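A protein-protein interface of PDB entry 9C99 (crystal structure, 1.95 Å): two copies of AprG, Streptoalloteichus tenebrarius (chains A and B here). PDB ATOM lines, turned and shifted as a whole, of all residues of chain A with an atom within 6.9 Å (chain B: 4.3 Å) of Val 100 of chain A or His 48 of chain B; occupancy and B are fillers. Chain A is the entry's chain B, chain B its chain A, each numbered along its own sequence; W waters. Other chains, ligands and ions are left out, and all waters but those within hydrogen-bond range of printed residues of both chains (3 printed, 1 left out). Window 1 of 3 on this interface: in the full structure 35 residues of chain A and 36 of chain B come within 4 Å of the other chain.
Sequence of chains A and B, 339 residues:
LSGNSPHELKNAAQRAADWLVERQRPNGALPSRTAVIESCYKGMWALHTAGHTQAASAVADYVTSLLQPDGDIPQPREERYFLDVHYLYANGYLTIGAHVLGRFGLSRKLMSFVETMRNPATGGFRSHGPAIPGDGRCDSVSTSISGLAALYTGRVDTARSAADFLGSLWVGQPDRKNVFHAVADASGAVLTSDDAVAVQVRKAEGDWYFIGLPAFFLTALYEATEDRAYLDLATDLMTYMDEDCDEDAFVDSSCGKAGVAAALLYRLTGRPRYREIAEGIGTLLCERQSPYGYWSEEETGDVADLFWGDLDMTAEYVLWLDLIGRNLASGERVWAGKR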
ATOM      1  N   TRP A  45      -9.299  -0.655  -3.807  1.00  0.00           N
ATOM      2  CA  TRP A  45      -9.221  -2.106  -3.913  1.00  0.00           C
ATOM      3  C   TRP A  45      -7.791  -2.591  -3.714  1.00  0.00           C
ATOM      4  O   TRP A  45      -7.552  -3.560  -2.993  1.00  0.00           O
ATOM      5  CB  TRP A  45      -9.755  -2.544  -5.273  1.00  0.00           C
ATOM      6  CG  TRP A  45     -10.019  -3.994  -5.411  1.00  0.00           C
ATOM      7  CD1 TRP A  45     -10.023  -4.932  -4.427  1.00  0.00           C
ATOM      8  CD2 TRP A  45     -10.308  -4.680  -6.627  1.00  0.00           C
ATOM      9  NE1 TRP A  45     -10.311  -6.160  -4.958  1.00  0.00           N
ATOM     10  CE2 TRP A  45     -10.493  -6.031  -6.307  1.00  0.00           C
ATOM     11  CE3 TRP A  45     -10.449  -4.273  -7.957  1.00  0.00           C
ATOM     12  CZ2 TRP A  45     -10.796  -6.986  -7.265  1.00  0.00           C
ATOM     13  CZ3 TRP A  45     -10.756  -5.228  -8.916  1.00  0.00           C
ATOM     14  CH2 TRP A  45     -10.914  -6.561  -8.565  1.00  0.00           C
ATOM     15  N   HIS A  48      -6.653  -2.277  -0.105  1.00  0.00           N
ATOM     16  CA  HIS A  48      -7.354  -3.193   0.774  1.00  0.00           C
ATOM     17  C   HIS A  48      -6.784  -4.608   0.648  1.00  0.00           C
ATOM     18  O   HIS A  48      -6.558  -5.276   1.666  1.00  0.00           O
ATOM     19  CB  HIS A  48      -8.859  -3.138   0.481  1.00  0.00           C
ATOM     20  CG  HIS A  48      -9.689  -3.934   1.437  1.00  0.00           C
ATOM     21  ND1 HIS A  48     -11.064  -3.942   1.401  1.00  0.00           N
ATOM     22  CD2 HIS A  48      -9.338  -4.743   2.464  1.00  0.00           C
ATOM     23  CE1 HIS A  48     -11.522  -4.727   2.362  1.00  0.00           C
ATOM     24  NE2 HIS A  48     -10.495  -5.228   3.016  1.00  0.00           N
ATOM     25  N   THR A  49      -6.495  -5.078  -0.581  1.00  0.00           N
ATOM     26  CA  THR A  49      -5.917  -6.420  -0.693  1.00  0.00           C
ATOM     27  C   THR A  49      -4.565  -6.509  -0.006  1.00  0.00           C
ATOM     28  O   THR A  49      -4.162  -7.595   0.434  1.00  0.00           O
ATOM     29  CB  THR A  49      -5.771  -6.873  -2.145  1.00  0.00           C
ATOM     30  OG1 THR A  49      -4.583  -6.306  -2.715  1.00  0.00           O
ATOM     31  CG2 THR A  49      -6.963  -6.460  -2.944  1.00  0.00           C
ATOM     32  N   ALA A  50      -3.850  -5.402   0.090  1.00  0.00           N
ATOM     33  CA  ALA A  50      -2.585  -5.423   0.813  1.00  0.00           C
ATOM     34  C   ALA A  50      -2.774  -5.287   2.323  1.00  0.00           C
ATOM     35  O   ALA A  50      -1.783  -5.204   3.045  1.00  0.00           O
ATOM     36  CB  ALA A  50      -1.672  -4.305   0.304  1.00  0.00           C
ATOM     37  N   GLY A  51      -4.019  -5.259   2.814  1.00  0.00           N
ATOM     38  CA  GLY A  51      -4.269  -5.097   4.232  1.00  0.00           C
ATOM     39  C   GLY A  51      -4.090  -3.695   4.771  1.00  0.00           C
ATOM     40  O   GLY A  51      -4.195  -3.498   5.991  1.00  0.00           O
ATOM     41  N   HIS A  52      -3.816  -2.718   3.911  1.00  0.00           N
ATOM     42  CA  HIS A  52      -3.735  -1.310   4.310  1.00  0.00           C
ATOM     43  C   HIS A  52      -5.139  -0.693   4.318  1.00  0.00           C
ATOM     44  O   HIS A  52      -5.480   0.175   3.511  1.00  0.00           O
ATOM     45  CB  HIS A  52      -2.820  -0.557   3.357  1.00  0.00           C
ATOM     46  CG  HIS A  52      -1.361  -0.779   3.618  1.00  0.00           C
ATOM     47  ND1 HIS A  52      -0.722  -0.266   4.727  1.00  0.00           N
ATOM     48  CD2 HIS A  52      -0.417  -1.450   2.912  1.00  0.00           C
ATOM     49  CE1 HIS A  52       0.557  -0.604   4.693  1.00  0.00           C
ATOM     50  NE2 HIS A  52       0.768  -1.328   3.605  1.00  0.00           N
ATOM     51  N   THR A  53      -5.967  -1.155   5.261  1.00  0.00           N
ATOM     52  CA  THR A  53      -7.370  -0.769   5.202  1.00  0.00           C
ATOM     53  C   THR A  53      -7.609   0.667   5.670  1.00  0.00           C
ATOM     54  O   THR A  53      -8.592   1.284   5.255  1.00  0.00           O
ATOM     55  CB  THR A  53      -8.229  -1.714   6.023  1.00  0.00           C
ATOM     56  OG1 THR A  53      -7.740  -1.737   7.375  1.00  0.00           O
ATOM     57  CG2 THR A  53      -8.194  -3.112   5.399  1.00  0.00           C
ATOM     58  N   THR A  95     -16.180   1.302  -7.749  1.00  0.00           N
ATOM     59  CA  THR A  95     -17.314   0.569  -7.188  1.00  0.00           C
ATOM     60  C   THR A  95     -16.852  -0.650  -6.408  1.00  0.00           C
ATOM     61  O   THR A  95     -17.318  -0.900  -5.288  1.00  0.00           O
ATOM     62  CB  THR A  95     -18.252   0.119  -8.308  1.00  0.00           C
ATOM     63  OG1 THR A  95     -18.667   1.249  -9.065  1.00  0.00           O
ATOM     64  CG2 THR A  95     -19.465  -0.591  -7.746  1.00  0.00           C
ATOM     65  N   ILE A  96     -15.963  -1.452  -7.021  1.00  0.00           N
ATOM     66  CA  ILE A  96     -15.488  -2.691  -6.410  1.00  0.00           C
ATOM     67  C   ILE A  96     -14.765  -2.390  -5.110  1.00  0.00           C
ATOM     68  O   ILE A  96     -14.962  -3.069  -4.088  1.00  0.00           O
ATOM     69  CB  ILE A  96     -14.564  -3.451  -7.390  1.00  0.00           C
ATOM     70  CG1 ILE A  96     -15.369  -3.969  -8.584  1.00  0.00           C
ATOM     71  CG2 ILE A  96     -13.823  -4.589  -6.675  1.00  0.00           C
ATOM     72  CD1 ILE A  96     -14.522  -4.532  -9.733  1.00  0.00           C
ATOM     73  N   GLY A  97     -13.870  -1.399  -5.146  1.00  0.00           N
ATOM     74  CA  GLY A  97     -13.089  -1.081  -3.962  1.00  0.00           C
ATOM     75  C   GLY A  97     -13.965  -0.584  -2.827  1.00  0.00           C
ATOM     76  O   GLY A  97     -13.771  -0.958  -1.665  1.00  0.00           O
ATOM     77  N   ALA A  98     -14.949   0.255  -3.152  1.00  0.00           N
ATOM     78  CA  ALA A  98     -15.888   0.723  -2.142  1.00  0.00           C
ATOM     79  C   ALA A  98     -16.678  -0.436  -1.556  1.00  0.00           C
ATOM     80  O   ALA A  98     -16.859  -0.516  -0.337  1.00  0.00           O
ATOM     81  CB  ALA A  98     -16.845   1.767  -2.728  1.00  0.00           C
ATOM     82  N   HIS A  99     -17.168  -1.346  -2.415  1.00  0.00           N
ATOM     83  CA  HIS A  99     -17.999  -2.439  -1.921  1.00  0.00           C
ATOM     84  C   HIS A  99     -17.209  -3.376  -1.010  1.00  0.00           C
ATOM     85  O   HIS A  99     -17.681  -3.753   0.068  1.00  0.00           O
ATOM     86  CB  HIS A  99     -18.603  -3.239  -3.076  1.00  0.00           C
ATOM     87  CG  HIS A  99     -19.615  -4.237  -2.619  1.00  0.00           C
ATOM     88  ND1 HIS A  99     -20.933  -3.899  -2.381  1.00  0.00           N
ATOM     89  CD2 HIS A  99     -19.498  -5.548  -2.297  1.00  0.00           C
ATOM     90  CE1 HIS A  99     -21.590  -4.970  -1.970  1.00  0.00           C
ATOM     91  NE2 HIS A  99     -20.742  -5.981  -1.906  1.00  0.00           N
ATOM     92  N   VAL A 100     -15.998  -3.756  -1.419  1.00  0.00           N
ATOM     93  CA  VAL A 100     -15.207  -4.680  -0.601  1.00  0.00           C
ATOM     94  C   VAL A 100     -14.824  -4.050   0.736  1.00  0.00           C
ATOM     95  O   VAL A 100     -14.694  -4.756   1.748  1.00  0.00           O
ATOM     96  CB  VAL A 100     -13.990  -5.162  -1.412  1.00  0.00           C
ATOM     97  CG1 VAL A 100     -13.029  -5.958  -0.560  1.00  0.00           C
ATOM     98  CG2 VAL A 100     -14.482  -6.028  -2.578  1.00  0.00           C
ATOM     99  N   LEU A 101     -14.676  -2.719   0.784  1.00  0.00           N
ATOM    100  CA  LEU A 101     -14.440  -2.015   2.040  1.00  0.00           C
ATOM    101  C   LEU A 101     -15.682  -1.916   2.926  1.00  0.00           C
ATOM    102  O   LEU A 101     -15.571  -1.428   4.051  1.00  0.00           O
ATOM    103  CB  LEU A 101     -13.923  -0.597   1.764  1.00  0.00           C
ATOM    104  CG  LEU A 101     -12.424  -0.415   1.558  1.00  0.00           C
ATOM    105  CD1 LEU A 101     -12.162   1.014   1.093  1.00  0.00           C
ATOM    106  CD2 LEU A 101     -11.605  -0.765   2.826  1.00  0.00           C
ATOM    107  N   GLY A 102     -16.853  -2.353   2.467  1.00  0.00           N
ATOM    108  CA  GLY A 102     -18.063  -2.141   3.243  1.00  0.00           C
ATOM    109  C   GLY A 102     -18.638  -0.744   3.163  1.00  0.00           C
ATOM    110  O   GLY A 102     -19.543  -0.409   3.939  1.00  0.00           O
ATOM    111  N   ARG A 103     -18.125   0.099   2.267  1.00  0.00           N
ATOM    112  CA  ARG A 103     -18.698   1.430   2.052  1.00  0.00           C
ATOM    113  C   ARG A 103     -19.876   1.269   1.096  1.00  0.00           C
ATOM    114  O   ARG A 103     -19.816   1.608  -0.086  1.00  0.00           O
ATOM    115  CB  ARG A 103     -17.662   2.393   1.496  1.00  0.00           C
ATOM    116  CG  ARG A 103     -16.514   2.668   2.432  1.00  0.00           C
ATOM    117  CD  ARG A 103     -16.893   3.716   3.455  1.00  0.00           C
ATOM    118  NE  ARG A 103     -15.727   4.096   4.248  1.00  0.00           N
ATOM    119  CZ  ARG A 103     -15.141   5.286   4.187  1.00  0.00           C
ATOM    120  NH1 ARG A 103     -15.618   6.220   3.371  1.00  0.00           N
ATOM    121  NH2 ARG A 103     -14.087   5.541   4.952  1.00  0.00           N
ATOM    122  N   PHE A 104     -20.952   0.697   1.635  1.00  0.00           N
ATOM    123  CA  PHE A 104     -22.057   0.246   0.801  1.00  0.00           C
ATOM    124  C   PHE A 104     -22.842   1.407   0.207  1.00  0.00           C
ATOM    125  O   PHE A 104     -23.475   1.238  -0.835  1.00  0.00           O
ATOM    126  CB  PHE A 104     -22.997  -0.653   1.606  1.00  0.00           C
ATOM    127  CG  PHE A 104     -22.383  -1.940   2.063  1.00  0.00           C
ATOM    128  CD1 PHE A 104     -21.662  -2.737   1.181  1.00  0.00           C
ATOM    129  CD2 PHE A 104     -22.522  -2.358   3.391  1.00  0.00           C
ATOM    130  CE1 PHE A 104     -21.113  -3.914   1.602  1.00  0.00           C
ATOM    131  CE2 PHE A 104     -21.960  -3.543   3.816  1.00  0.00           C
ATOM    132  CZ  PHE A 104     -21.257  -4.317   2.922  1.00  0.00           C
ATOM    133  N   SER A 107     -20.667   2.378  -2.871  1.00  0.00           N
ATOM    134  CA  SER A 107     -20.747   1.403  -3.961  1.00  0.00           C
ATOM    135  C   SER A 107     -22.137   1.378  -4.575  1.00  0.00           C
ATOM    136  O   SER A 107     -22.266   1.260  -5.795  1.00  0.00           O
ATOM    137  CB  SER A 107     -20.325   0.004  -3.492  1.00  0.00           C
ATOM    138  OG  SER A 107     -21.286  -0.599  -2.643  1.00  0.00           O
ATOM    139  N   TYR A 152     -19.391  -8.000  -8.004  1.00  0.00           N
ATOM    140  CA  TYR A 152     -19.058  -7.673  -6.619  1.00  0.00           C
ATOM    141  C   TYR A 152     -20.258  -7.072  -5.877  1.00  0.00           C
ATOM    142  O   TYR A 152     -20.429  -7.322  -4.681  1.00  0.00           O
ATOM    143  CB  TYR A 152     -17.846  -6.729  -6.569  1.00  0.00           C
ATOM    144  CG  TYR A 152     -16.522  -7.475  -6.565  1.00  0.00           C
ATOM    145  CD1 TYR A 152     -16.027  -8.021  -5.384  1.00  0.00           C
ATOM    146  CD2 TYR A 152     -15.798  -7.681  -7.741  1.00  0.00           C
ATOM    147  CE1 TYR A 152     -14.833  -8.737  -5.363  1.00  0.00           C
ATOM    148  CE2 TYR A 152     -14.588  -8.377  -7.731  1.00  0.00           C
ATOM    149  CZ  TYR A 152     -14.118  -8.903  -6.536  1.00  0.00           C
ATOM    150  OH  TYR A 152     -12.948  -9.610  -6.484  1.00  0.00           O
ATOM    151  N   ASP A 322      -1.369  -9.614  -6.409  1.00  0.00           N
ATOM    152  CA  ASP A 322      -2.119 -10.268  -5.345  1.00  0.00           C
ATOM    153  C   ASP A 322      -3.088 -11.307  -5.901  1.00  0.00           C
ATOM    154  O   ASP A 322      -3.127 -12.451  -5.420  1.00  0.00           O
ATOM    155  CB  ASP A 322      -2.877  -9.251  -4.499  1.00  0.00           C
ATOM    156  CG  ASP A 322      -3.659  -9.924  -3.400  1.00  0.00           C
ATOM    157  OD1 ASP A 322      -4.805 -10.373  -3.649  1.00  0.00           O
ATOM    158  OD2 ASP A 322      -3.098 -10.055  -2.300  1.00  0.00           O
ATOM    159  N   ARG A 326      -2.865 -15.353  -5.254  1.00  0.00           N
ATOM    160  CA  ARG A 326      -3.718 -16.202  -4.435  1.00  0.00           C
ATOM    161  C   ARG A 326      -4.420 -17.277  -5.256  1.00  0.00           C
ATOM    162  O   ARG A 326      -4.663 -18.384  -4.741  1.00  0.00           O
ATOM    163  CB  ARG A 326      -4.719 -15.357  -3.656  1.00  0.00           C
ATOM    164  CG  ARG A 326      -5.616 -14.552  -4.490  1.00  0.00           C
ATOM    165  CD  ARG A 326      -6.071 -13.381  -3.649  1.00  0.00           C
ATOM    166  NE  ARG A 326      -7.465 -13.075  -3.868  1.00  0.00           N
ATOM    167  CZ  ARG A 326      -8.010 -11.885  -3.642  1.00  0.00           C
ATOM    168  NH1 ARG A 326      -9.301 -11.705  -3.857  1.00  0.00           N
ATOM    169  NH2 ARG A 326      -7.263 -10.873  -3.224  1.00  0.00           N
ATOM    170  N   MET B  44     -11.554 -16.335   6.813  1.00  0.00           N
ATOM    171  CA  MET B  44     -11.418 -15.764   5.473  1.00  0.00           C
ATOM    172  C   MET B  44     -11.454 -14.242   5.543  1.00  0.00           C
ATOM    173  O   MET B  44     -10.553 -13.562   5.035  1.00  0.00           O
ATOM    174  CB  MET B  44     -12.515 -16.288   4.536  1.00  0.00           C
ATOM    175  CG  MET B  44     -12.224 -17.662   3.919  1.00  0.00           C
ATOM    176  SD  MET B  44     -13.543 -18.103   2.743  1.00  0.00           S
ATOM    177  CE  MET B  44     -14.882 -18.358   3.880  1.00  0.00           C
ATOM    178  N   TRP B  45     -12.483 -13.688   6.199  1.00  0.00           N
ATOM    179  CA  TRP B  45     -12.659 -12.236   6.235  1.00  0.00           C
ATOM    180  C   TRP B  45     -11.561 -11.571   7.064  1.00  0.00           C
ATOM    181  O   TRP B  45     -10.975 -10.568   6.647  1.00  0.00           O
ATOM    182  CB  TRP B  45     -14.051 -11.910   6.792  1.00  0.00           C
ATOM    183  CG  TRP B  45     -14.508 -10.452   6.739  1.00  0.00           C
ATOM    184  CD1 TRP B  45     -13.946  -9.409   6.032  1.00  0.00           C
ATOM    185  CD2 TRP B  45     -15.646  -9.908   7.414  1.00  0.00           C
ATOM    186  NE1 TRP B  45     -14.668  -8.254   6.248  1.00  0.00           N
ATOM    187  CE2 TRP B  45     -15.709  -8.531   7.098  1.00  0.00           C
ATOM    188  CE3 TRP B  45     -16.618 -10.456   8.266  1.00  0.00           C
ATOM    189  CZ2 TRP B  45     -16.719  -7.694   7.589  1.00  0.00           C
ATOM    190  CZ3 TRP B  45     -17.624  -9.626   8.756  1.00  0.00           C
ATOM    191  CH2 TRP B  45     -17.658  -8.253   8.423  1.00  0.00           C
ATOM    192  N   ALA B  46     -11.251 -12.128   8.241  1.00  0.00           N
ATOM    193  CA  ALA B  46     -10.202 -11.542   9.079  1.00  0.00           C
ATOM    194  C   ALA B  46      -8.861 -11.503   8.346  1.00  0.00           C
ATOM    195  O   ALA B  46      -8.214 -10.453   8.281  1.00  0.00           O
ATOM    196  CB  ALA B  46     -10.084 -12.315  10.397  1.00  0.00           C
ATOM    197  N   LEU B  47      -8.434 -12.635   7.766  1.00  0.00           N
ATOM    198  CA  LEU B  47      -7.131 -12.671   7.098  1.00  0.00           C
ATOM    199  C   LEU B  47      -7.108 -11.784   5.871  1.00  0.00           C
ATOM    200  O   LEU B  47      -6.053 -11.240   5.514  1.00  0.00           O
ATOM    201  CB  LEU B  47      -6.773 -14.101   6.689  1.00  0.00           C
ATOM    202  CG  LEU B  47      -6.618 -14.942   7.942  1.00  0.00           C
ATOM    203  CD1 LEU B  47      -6.534 -16.377   7.510  1.00  0.00           C
ATOM    204  CD2 LEU B  47      -5.377 -14.487   8.751  1.00  0.00           C
ATOM    205  N   HIS B  48      -8.255 -11.628   5.205  1.00  0.00           N
ATOM    206  CA  HIS B  48      -8.302 -10.711   4.069  1.00  0.00           C
ATOM    207  C   HIS B  48      -8.087  -9.262   4.520  1.00  0.00           C
ATOM    208  O   HIS B  48      -7.304  -8.526   3.900  1.00  0.00           O
ATOM    209  CB  HIS B  48      -9.629 -10.860   3.311  1.00  0.00           C
ATOM    210  CG  HIS B  48      -9.768  -9.910   2.157  1.00  0.00           C
ATOM    211  ND1 HIS B  48      -9.379 -10.233   0.876  1.00  0.00           N
ATOM    212  CD2 HIS B  48     -10.231  -8.636   2.095  1.00  0.00           C
ATOM    213  CE1 HIS B  48      -9.590  -9.206   0.073  1.00  0.00           C
ATOM    214  NE2 HIS B  48     -10.117  -8.224   0.785  1.00  0.00           N
ATOM    215  N   THR B  49      -8.726  -8.844   5.627  1.00  0.00           N
ATOM    216  CA  THR B  49      -8.507  -7.480   6.095  1.00  0.00           C
ATOM    217  C   THR B  49      -7.062  -7.243   6.489  1.00  0.00           C
ATOM    218  O   THR B  49      -6.601  -6.107   6.414  1.00  0.00           O
ATOM    219  CB  THR B  49      -9.416  -7.083   7.280  1.00  0.00           C
ATOM    220  OG1 THR B  49      -8.910  -7.599   8.521  1.00  0.00           O
ATOM    221  CG2 THR B  49     -10.838  -7.554   7.065  1.00  0.00           C
ATOM    222  N   ALA B  50      -6.339  -8.280   6.900  1.00  0.00           N
ATOM    223  CA  ALA B  50      -4.928  -8.121   7.224  1.00  0.00           C
ATOM    224  C   ALA B  50      -4.016  -8.188   6.002  1.00  0.00           C
ATOM    225  O   ALA B  50      -2.786  -8.137   6.150  1.00  0.00           O
ATOM    226  CB  ALA B  50      -4.524  -9.183   8.226  1.00  0.00           C
ATOM    227  N   GLY B  51      -4.572  -8.301   4.804  1.00  0.00           N
ATOM    228  CA  GLY B  51      -3.750  -8.396   3.622  1.00  0.00           C
ATOM    229  C   GLY B  51      -3.173  -9.773   3.378  1.00  0.00           C
ATOM    230  O   GLY B  51      -2.434  -9.951   2.406  1.00  0.00           O
ATOM    231  N   THR B  53      -3.957 -12.493   1.850  1.00  0.00           N
ATOM    232  CA  THR B  53      -4.969 -13.011   0.937  1.00  0.00           C
ATOM    233  C   THR B  53      -4.707 -14.452   0.519  1.00  0.00           C
ATOM    234  O   THR B  53      -5.661 -15.178   0.207  1.00  0.00           O
ATOM    235  CB  THR B  53      -5.077 -12.109  -0.297  1.00  0.00           C
ATOM    236  OG1 THR B  53      -3.767 -11.905  -0.847  1.00  0.00           O
ATOM    237  CG2 THR B  53      -5.691 -10.751   0.124  1.00  0.00           C
ATOM    238  N   ALA B  56      -6.066 -16.385   3.452  1.00  0.00           N
ATOM    239  CA  ALA B  56      -7.523 -16.297   3.394  1.00  0.00           C
ATOM    240  C   ALA B  56      -8.087 -17.199   2.303  1.00  0.00           C
ATOM    241  O   ALA B  56      -9.081 -17.903   2.521  1.00  0.00           O
ATOM    242  CB  ALA B  56      -7.958 -14.845   3.161  1.00  0.00           C
ATOM    243  N   VAL B 100     -15.943 -11.262  -0.409  1.00  0.00           N
ATOM    244  CA  VAL B 100     -14.932 -10.224  -0.559  1.00  0.00           C
ATOM    245  C   VAL B 100     -13.673 -10.775  -1.217  1.00  0.00           C
ATOM    246  O   VAL B 100     -12.925 -10.011  -1.836  1.00  0.00           O
ATOM    247  CB  VAL B 100     -14.616  -9.547   0.794  1.00  0.00           C
ATOM    248  CG1 VAL B 100     -15.890  -8.983   1.429  1.00  0.00           C
ATOM    249  CG2 VAL B 100     -13.926 -10.483   1.735  1.00  0.00           C
ATOM    250  N   LEU B 101     -13.426 -12.085  -1.124  1.00  0.00           N
ATOM    251  CA  LEU B 101     -12.316 -12.716  -1.839  1.00  0.00           C
ATOM    252  C   LEU B 101     -12.606 -12.945  -3.319  1.00  0.00           C
ATOM    253  O   LEU B 101     -11.741 -13.470  -4.033  1.00  0.00           O
ATOM    254  CB  LEU B 101     -11.979 -14.060  -1.203  1.00  0.00           C
ATOM    255  CG  LEU B 101     -11.075 -14.012   0.026  1.00  0.00           C
ATOM    256  CD1 LEU B 101     -11.083 -15.385   0.698  1.00  0.00           C
ATOM    257  CD2 LEU B 101      -9.653 -13.581  -0.375  1.00  0.00           C
ATOM    258  N   TYR B 152     -23.316  -7.771   1.974  1.00  0.00           N
ATOM    259  CA  TYR B 152     -22.086  -7.965   1.207  1.00  0.00           C
ATOM    260  C   TYR B 152     -22.364  -8.595  -0.157  1.00  0.00           C
ATOM    261  O   TYR B 152     -21.654  -8.306  -1.130  1.00  0.00           O
ATOM    262  CB  TYR B 152     -21.077  -8.807   2.008  1.00  0.00           C
ATOM    263  CG  TYR B 152     -20.169  -7.928   2.862  1.00  0.00           C
ATOM    264  CD1 TYR B 152     -19.094  -7.259   2.290  1.00  0.00           C
ATOM    265  CD2 TYR B 152     -20.429  -7.725   4.224  1.00  0.00           C
ATOM    266  CE1 TYR B 152     -18.266  -6.434   3.048  1.00  0.00           C
ATOM    267  CE2 TYR B 152     -19.615  -6.891   4.996  1.00  0.00           C
ATOM    268  CZ  TYR B 152     -18.546  -6.240   4.399  1.00  0.00           C
ATOM    269  OH  TYR B 152     -17.732  -5.405   5.140  1.00  0.00           O
HETATM  270  O   HOH W   1     -11.479  -9.684  -4.007  1.00  0.00           O
HETATM  271  O   HOH W   2      -1.794 -13.031  -2.949  1.00  0.00           O
HETATM  272  O   HOH W   3      -9.632 -15.081  -5.344  1.00  0.00           O
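The side-chain carboxylate (OD2) of Asp 322 of chain A lies within hydrogen-bond range of the side-chain hydroxyl (OG1) of Thr 53 of chain B (2.4 Å). NH1 of Arg 326 of chain A sits at hydrogen-bond distance from O of Leu 101 of chain B, 3.0 Å away. O of Tyr 152 of chain B lies within hydrogen-bond range of NE2 of His 99 of chain A (2.6 Å).
The side-chain hydroxyl (OG1) of Thr 49 of chain B sits at hydrogen-bond distance from the backbone carbonyl oxygen (O) of Ala 46 of chain B, at 2.9 Å. A ring nitrogen (ND1) of His 99 of chain A sits at hydrogen-bond distance from the side-chain hydroxyl of Ser 107 of chain A. A ring nitrogen (NE2) of His 99 of chain A is in hydrogen-bond range of the backbone carbonyl oxygen of Tyr 152 of chain A. O of Phe 104 of chain A sits at hydrogen-bond distance from OG of Ser 107 of chain A, 3.4 Å away. The side-chain carboxylate of Asp 322 of chain A is in salt-bridge range of the guanidinium group of Arg 326 of chain A, 2.5 Å away.
Gly 51 of chain B touches Thr 49 of chain A. Gly 51 of chain B touches Ala 50 of chain A (CA to C, 3.5 Å). Thr 49 of chain B touches Gly 51 of chain A (O to CA, 3.3 Å). Gly 51 of chain A touches Ala 50 of chain B. Gly 51 of chain A touches Gly 51 of chain B (N to CA, 3.3 Å). Thr 49 of chain B touches Thr 53 of chain A. Val 100 of chain A touches His 48 of chain B. Gly 102 of chain A touches Tyr 152 of chain B (CA to OH, 3.8 Å). Phe 104 of chain A touches Tyr 152 of chain B. O of Tyr 152 of chain A touches O of Tyr 152 of chain B, at 3.9 Å.
Val 100 of chain A touches one residue of chain B. Of the printed residues of chain A, His 48 of chain B touches His 48 (3.5 Å) and Val 100 (3.9 Å). Of the printed residues of chain A, Gly 51 of chain B touches Thr 49 (3.3 Å), Ala 50 (3.5 Å) and Gly 51 (3.3 Å). Of the printed residues of chain B, Asp 322 of chain A touches Thr 53 (2.4 Å). Printed residues of chain B within 4 Å of Arg 326 of chain A: Thr 53 and Leu 101. The nearest printed residue of chain A that does not touch Thr 49 of chain B is His 48 of chain A (4.3 Å).
Of the 21 printed residues of chain A, 12 touch a printed residue of chain B. Hydrophobic or aromatic side chains of chain A that line the printed part of chain B: His 48, His 99, Val 100 and Phe 104. Hydrophobic or aromatic side chains of chain B that line the printed part of chain A: His 48, Leu 101 and Tyr 152. Among the printed residues, 16 pairs touch across the chains. Among the printed residues, no Asp or Glu carboxylate lies within 4 Å of a Lys or Arg side-chain nitrogen of the other chain.
Thr 49 of chain A touches Gly 51 of chain B, and with the chains exchanged Gly 51 of chain A touches Thr 49 of chain B. Ala 50 of chain A touches Gly 51 of chain B, and with the chains exchanged Gly 51 of chain A touches Ala 50 of chain B. Val 100 of chain A touches His 48 of chain B, but with the chains exchanged His 48 of chain A does not touch Val 100 of chain B (5.9 Å). Tyr 152 of chain B touches its own counterpart, Tyr 152 of chain A. Positions printed for both chains: 45, 48, 49, 50, 51, 53, 100, 101 and 152.
Water W1 lies within hydrogen-bond range of O of Val 100 of chain B, OH of Tyr 152 of chain A and NH1 of Arg 326 of chain A. Water W2 lies within hydrogen-bond range of O of Asp 322 of chain A (2.9 Å), OG1 of Thr 53 of chain B (3.1 Å) and N of Arg 326 of chain A (3.4 Å). Water W3 lies within hydrogen-bond range of the backbone carbonyl oxygen (O) of Leu 101 of chain B and the guanidinium group (NE) of Arg 326 of chain A.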
